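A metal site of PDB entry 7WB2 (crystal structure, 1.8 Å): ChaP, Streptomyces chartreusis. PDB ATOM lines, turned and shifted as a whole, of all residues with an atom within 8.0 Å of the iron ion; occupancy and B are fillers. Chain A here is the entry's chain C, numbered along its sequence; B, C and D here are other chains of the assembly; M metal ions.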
ATOM      1  N   ALA A   3       6.776  15.958  25.025  1.00  0.00           N
ATOM      2  CA  ALA A   3       8.075  15.809  24.380  1.00  0.00           C
ATOM      3  C   ALA A   3       9.137  16.757  24.905  1.00  0.00           C
ATOM      4  O   ALA A   3      10.308  16.591  24.546  1.00  0.00           O
ATOM      5  CB  ALA A   3       7.946  15.994  22.864  1.00  0.00           C
ATOM      6  N   VAL A   4       8.787  17.752  25.712  1.00  0.00           N
ATOM      7  CA  VAL A   4       9.774  18.733  26.147  1.00  0.00           C
ATOM      8  C   VAL A   4      10.783  18.070  27.063  1.00  0.00           C
ATOM      9  O   VAL A   4      10.417  17.329  27.976  1.00  0.00           O
ATOM     10  CB  VAL A   4       9.103  19.919  26.852  1.00  0.00           C
ATOM     11  CG1 VAL A   4      10.078  21.076  26.986  1.00  0.00           C
ATOM     12  CG2 VAL A   4       7.900  20.353  26.050  1.00  0.00           C
ATOM     13  N   GLU A   5      12.067  18.400  26.861  1.00  0.00           N
ATOM     14  CA  GLU A   5      13.157  17.873  27.657  1.00  0.00           C
ATOM     15  C   GLU A   5      13.826  18.988  28.464  1.00  0.00           C
ATOM     16  O   GLU A   5      13.867  20.147  28.046  1.00  0.00           O
ATOM     17  CB  GLU A   5      14.210  17.207  26.763  1.00  0.00           C
ATOM     18  CG  GLU A   5      13.590  16.228  25.781  1.00  0.00           C
ATOM     19  CD  GLU A   5      14.597  15.450  24.980  1.00  0.00           C
ATOM     20  OE1 GLU A   5      14.177  14.582  24.195  1.00  0.00           O
ATOM     21  OE2 GLU A   5      15.816  15.707  25.144  1.00  0.00           O
ATOM     22  N   LEU A   6      14.326  18.626  29.645  1.00  0.00           N
ATOM     23  CA  LEU A   6      15.185  19.511  30.414  1.00  0.00           C
ATOM     24  C   LEU A   6      16.605  19.323  29.896  1.00  0.00           C
ATOM     25  O   LEU A   6      17.203  18.259  30.049  1.00  0.00           O
ATOM     26  CB  LEU A   6      15.076  19.209  31.909  1.00  0.00           C
ATOM     27  CG  LEU A   6      15.908  20.114  32.809  1.00  0.00           C
ATOM     28  CD1 LEU A   6      15.347  21.528  32.828  1.00  0.00           C
ATOM     29  CD2 LEU A   6      15.925  19.537  34.213  1.00  0.00           C
ATOM     30  N   ASN A   7      17.136  20.369  29.259  1.00  0.00           N
ATOM     31  CA  ASN A   7      18.427  20.239  28.586  1.00  0.00           C
ATOM     32  C   ASN A   7      19.593  20.614  29.486  1.00  0.00           C
ATOM     33  O   ASN A   7      20.659  20.001  29.402  1.00  0.00           O
ATOM     34  CB  ASN A   7      18.453  21.096  27.325  1.00  0.00           C
ATOM     35  CG  ASN A   7      19.767  21.004  26.599  1.00  0.00           C
ATOM     36  OD1 ASN A   7      20.663  21.815  26.843  1.00  0.00           O
ATOM     37  ND2 ASN A   7      19.904  19.999  25.737  1.00  0.00           N
ATOM     38  N   ASN A  45      21.048  11.240  30.194  1.00  0.00           N
ATOM     39  CA  ASN A  45      19.733  11.474  29.608  1.00  0.00           C
ATOM     40  C   ASN A  45      19.580  12.881  29.011  1.00  0.00           C
ATOM     41  O   ASN A  45      18.609  13.574  29.298  1.00  0.00           O
ATOM     42  CB  ASN A  45      18.646  11.159  30.630  1.00  0.00           C
ATOM     43  CG  ASN A  45      18.847  11.856  31.995  1.00  0.00           C
ATOM     44  OD1 ASN A  45      19.970  11.968  32.488  1.00  0.00           O
ATOM     45  ND2 ASN A  45      17.737  12.262  32.610  1.00  0.00           N
ATOM     46  N   ASP A  46      20.521  13.291  28.157  1.00  0.00           N
ATOM     47  CA  ASP A  46      20.416  14.536  27.380  1.00  0.00           C
ATOM     48  C   ASP A  46      20.223  15.750  28.289  1.00  0.00           C
ATOM     49  O   ASP A  46      19.430  16.644  28.001  1.00  0.00           O
ATOM     50  CB  ASP A  46      19.299  14.438  26.334  1.00  0.00           C
ATOM     51  CG  ASP A  46      19.484  15.397  25.166  1.00  0.00           C
ATOM     52  OD1 ASP A  46      20.520  16.103  25.146  1.00  0.00           O
ATOM     53  OD2 ASP A  46      18.598  15.469  24.263  1.00  0.00           O
ATOM     54  N   VAL A  47      20.965  15.783  29.402  1.00  0.00           N
ATOM     55  CA  VAL A  47      20.847  16.858  30.380  1.00  0.00           C
ATOM     56  C   VAL A  47      22.210  17.108  31.027  1.00  0.00           C
ATOM     57  O   VAL A  47      22.995  16.183  31.227  1.00  0.00           O
ATOM     58  CB  VAL A  47      19.798  16.520  31.472  1.00  0.00           C
ATOM     59  CG1 VAL A  47      20.206  15.290  32.235  1.00  0.00           C
ATOM     60  CG2 VAL A  47      19.626  17.689  32.418  1.00  0.00           C
ATOM     61  N   ALA B   3      19.180   5.650  28.068  1.00  0.00           N
ATOM     62  CA  ALA B   3      19.014   7.069  27.812  1.00  0.00           C
ATOM     63  C   ALA B   3      19.266   7.461  26.365  1.00  0.00           C
ATOM     64  O   ALA B   3      19.168   8.651  26.045  1.00  0.00           O
ATOM     65  CB  ALA B   3      19.905   7.899  28.760  1.00  0.00           C
ATOM     66  N   VAL B   4      19.651   6.508  25.509  1.00  0.00           N
ATOM     67  CA  VAL B   4      20.030   6.796  24.119  1.00  0.00           C
ATOM     68  C   VAL B   4      18.800   7.245  23.349  1.00  0.00           C
ATOM     69  O   VAL B   4      17.740   6.629  23.448  1.00  0.00           O
ATOM     70  CB  VAL B   4      20.658   5.546  23.465  1.00  0.00           C
ATOM     71  CG1 VAL B   4      20.904   5.777  21.974  1.00  0.00           C
ATOM     72  CG2 VAL B   4      21.950   5.126  24.186  1.00  0.00           C
ATOM     73  N   GLU B   5      18.951   8.304  22.554  1.00  0.00           N
ATOM     74  CA  GLU B   5      17.848   8.818  21.767  1.00  0.00           C
ATOM     75  C   GLU B   5      18.119   8.653  20.272  1.00  0.00           C
ATOM     76  O   GLU B   5      19.275   8.673  19.843  1.00  0.00           O
ATOM     77  CB  GLU B   5      17.600  10.301  22.090  1.00  0.00           C
ATOM     78  CG  GLU B   5      17.292  10.549  23.561  1.00  0.00           C
ATOM     79  CD  GLU B   5      17.068  12.011  23.840  1.00  0.00           C
ATOM     80  OE1 GLU B   5      17.171  12.815  22.885  1.00  0.00           O
ATOM     81  OE2 GLU B   5      16.739  12.337  24.987  1.00  0.00           O
ATOM     82  N   LEU B   6      17.047   8.475  19.513  1.00  0.00           N
ATOM     83  CA  LEU B   6      17.137   8.530  18.059  1.00  0.00           C
ATOM     84  C   LEU B   6      17.040   9.992  17.637  1.00  0.00           C
ATOM     85  O   LEU B   6      15.975  10.596  17.732  1.00  0.00           O
ATOM     86  CB  LEU B   6      16.062   7.666  17.403  1.00  0.00           C
ATOM     87  CG  LEU B   6      16.103   7.709  15.879  1.00  0.00           C
ATOM     88  CD1 LEU B   6      17.403   7.137  15.372  1.00  0.00           C
ATOM     89  CD2 LEU B   6      14.936   6.946  15.313  1.00  0.00           C
ATOM     90  N   ASN B   7      18.149  10.552  17.135  1.00  0.00           N
ATOM     91  CA  ASN B   7      18.229  11.998  16.866  1.00  0.00           C
ATOM     92  C   ASN B   7      17.815  12.358  15.448  1.00  0.00           C
ATOM     93  O   ASN B   7      17.179  13.401  15.227  1.00  0.00           O
ATOM     94  CB  ASN B   7      19.639  12.523  17.142  1.00  0.00           C
ATOM     95  CG  ASN B   7      19.766  14.030  16.946  1.00  0.00           C
ATOM     96  OD1 ASN B   7      20.262  14.497  15.924  1.00  0.00           O
ATOM     97  ND2 ASN B   7      19.288  14.804  17.934  1.00  0.00           N
ATOM     98  N   ALA B  44       8.389  16.472  17.274  1.00  0.00           N
ATOM     99  CA  ALA B  44       8.486  17.110  18.578  1.00  0.00           C
ATOM    100  C   ALA B  44       9.427  16.390  19.541  1.00  0.00           C
ATOM    101  O   ALA B  44      10.023  17.040  20.403  1.00  0.00           O
ATOM    102  CB  ALA B  44       7.095  17.229  19.202  1.00  0.00           C
ATOM    103  N   ASN B  45       9.607  15.075  19.377  1.00  0.00           N
ATOM    104  CA  ASN B  45      10.354  14.281  20.361  1.00  0.00           C
ATOM    105  C   ASN B  45      11.841  14.203  20.025  1.00  0.00           C
ATOM    106  O   ASN B  45      12.427  13.130  19.973  1.00  0.00           O
ATOM    107  CB  ASN B  45       9.728  12.893  20.502  1.00  0.00           C
ATOM    108  CG  ASN B  45       9.481  12.188  19.150  1.00  0.00           C
ATOM    109  OD1 ASN B  45       9.135  12.831  18.164  1.00  0.00           O
ATOM    110  ND2 ASN B  45       9.571  10.859  19.139  1.00  0.00           N
ATOM    111  N   ASP B  46      12.461  15.372  19.794  1.00  0.00           N
ATOM    112  CA  ASP B  46      13.919  15.476  19.626  1.00  0.00           C
ATOM    113  C   ASP B  46      14.425  14.527  18.529  1.00  0.00           C
ATOM    114  O   ASP B  46      15.442  13.852  18.684  1.00  0.00           O
ATOM    115  CB  ASP B  46      14.656  15.225  20.941  1.00  0.00           C
ATOM    116  CG  ASP B  46      16.039  15.843  20.959  1.00  0.00           C
ATOM    117  OD1 ASP B  46      16.413  16.497  19.970  1.00  0.00           O
ATOM    118  OD2 ASP B  46      16.762  15.661  21.969  1.00  0.00           O
ATOM    119  N   VAL B  47      13.684  14.464  17.420  1.00  0.00           N
ATOM    120  CA  VAL B  47      14.056  13.627  16.287  1.00  0.00           C
ATOM    121  C   VAL B  47      13.576  14.294  15.011  1.00  0.00           C
ATOM    122  O   VAL B  47      12.523  14.947  14.983  1.00  0.00           O
ATOM    123  CB  VAL B  47      13.475  12.202  16.417  1.00  0.00           C
ATOM    124  CG1 VAL B  47      11.970  12.220  16.313  1.00  0.00           C
ATOM    125  CG2 VAL B  47      14.087  11.271  15.366  1.00  0.00           C
ATOM    126  N   ALA C  44      10.366  14.990  29.414  1.00  0.00           N
ATOM    127  CA  ALA C  44      10.385  13.795  28.578  1.00  0.00           C
ATOM    128  C   ALA C  44      11.662  12.974  28.737  1.00  0.00           C
ATOM    129  O   ALA C  44      11.642  11.757  28.512  1.00  0.00           O
ATOM    130  CB  ALA C  44      10.191  14.168  27.110  1.00  0.00           C
ATOM    131  N   ASN C  45      12.789  13.610  29.090  1.00  0.00           N
ATOM    132  CA  ASN C  45      14.047  12.870  29.152  1.00  0.00           C
ATOM    133  C   ASN C  45      14.326  12.328  30.558  1.00  0.00           C
ATOM    134  O   ASN C  45      15.451  12.402  31.066  1.00  0.00           O
ATOM    135  CB  ASN C  45      15.203  13.725  28.654  1.00  0.00           C
ATOM    136  CG  ASN C  45      15.237  15.109  29.285  1.00  0.00           C
ATOM    137  OD1 ASN C  45      14.212  15.680  29.587  1.00  0.00           O
ATOM    138  ND2 ASN C  45      16.432  15.663  29.421  1.00  0.00           N
ATOM    139  N   LEU C  68      14.326  22.082  26.096  1.00  0.00           N
ATOM    140  CA  LEU C  68      14.509  21.831  24.671  1.00  0.00           C
ATOM    141  C   LEU C  68      13.192  21.450  24.012  1.00  0.00           C
ATOM    142  O   LEU C  68      12.507  20.524  24.450  1.00  0.00           O
ATOM    143  CB  LEU C  68      15.528  20.723  24.437  1.00  0.00           C
ATOM    144  CG  LEU C  68      15.783  20.458  22.955  1.00  0.00           C
ATOM    145  CD1 LEU C  68      16.771  21.410  22.349  1.00  0.00           C
ATOM    146  CD2 LEU C  68      16.262  19.015  22.835  1.00  0.00           C
ATOM    147  N   ARG C 124      17.123  22.890  18.976  1.00  0.00           N
ATOM    148  CA  ARG C 124      18.366  22.242  18.529  1.00  0.00           C
ATOM    149  C   ARG C 124      18.057  21.499  17.238  1.00  0.00           C
ATOM    150  O   ARG C 124      17.989  20.268  17.209  1.00  0.00           O
ATOM    151  CB  ARG C 124      18.909  21.290  19.600  1.00  0.00           C
ATOM    152  N   ALA D  44      15.102   6.233  23.870  1.00  0.00           N
ATOM    153  CA  ALA D  44      14.594   6.917  25.058  1.00  0.00           C
ATOM    154  C   ALA D  44      13.621   8.036  24.699  1.00  0.00           C
ATOM    155  O   ALA D  44      12.776   8.393  25.528  1.00  0.00           O
ATOM    156  CB  ALA D  44      15.748   7.461  25.893  1.00  0.00           C
ATOM    157  N   ASN D  45      13.723   8.615  23.508  1.00  0.00           N
ATOM    158  CA  ASN D  45      12.872   9.766  23.171  1.00  0.00           C
ATOM    159  C   ASN D  45      11.592   9.324  22.472  1.00  0.00           C
ATOM    160  O   ASN D  45      11.163   9.931  21.496  1.00  0.00           O
ATOM    161  CB  ASN D  45      13.643  10.773  22.336  1.00  0.00           C
ATOM    162  CG  ASN D  45      14.292  10.154  21.105  1.00  0.00           C
ATOM    163  OD1 ASN D  45      14.761   9.006  21.142  1.00  0.00           O
ATOM    164  ND2 ASN D  45      14.352  10.912  20.009  1.00  0.00           N
ATOM    165  N   LEU D  68      22.041   9.824  19.572  1.00  0.00           N
ATOM    166  CA  LEU D  68      22.553  10.859  20.449  1.00  0.00           C
ATOM    167  C   LEU D  68      22.818  10.274  21.813  1.00  0.00           C
ATOM    168  O   LEU D  68      21.935   9.650  22.419  1.00  0.00           O
ATOM    169  CB  LEU D  68      21.556  12.024  20.538  1.00  0.00           C
HETATM  170 FE    FE M   1      16.888  14.771  23.682  1.00  0.00          FE
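The backbone NH (N) of Leu 68 of chain D sits at hydrogen-bond distance from the backbone carbonyl oxygen (O) of Glu 5 of chain B (3.0 Å). The side-chain amide nitrogen (ND2) of Asn 45 of chain D lies within hydrogen-bond range of the backbone carbonyl oxygen (O) of Asp 46 of chain B (3.4 Å). N of Leu 68 of chain C sits at hydrogen-bond distance from O of Glu 5 of chain A (2.8 Å). The backbone carbonyl oxygen (O) of Asp 46 of chain A lies within hydrogen-bond range of the side-chain amide nitrogen (ND2) of Asn 45 of chain C (3.5 Å).
The iron ion is bound by the side-chain carboxylate (OD2) of Asp 46 of chain B (1.9 Å), the side-chain carboxylate (OD2) of Asp 46 of chain A (1.9 Å), the side-chain carboxylate (OE2) of Glu 5 of chain A (2.0 Å) and the side-chain carboxylate (OE1) of Glu 5 of chain B (2.1 Å). The iron ion has four donor atoms within binding distance. Slightly farther from the iron ion lies OE1 of Glu 5 of chain A (2.8 Å). Slightly farther from the iron ion lies the side-chain carboxylate (OE2) of Glu 5 of chain B (2.8 Å).
Of the 24 residues printed, 4 come within 4 Å of the iron ion.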
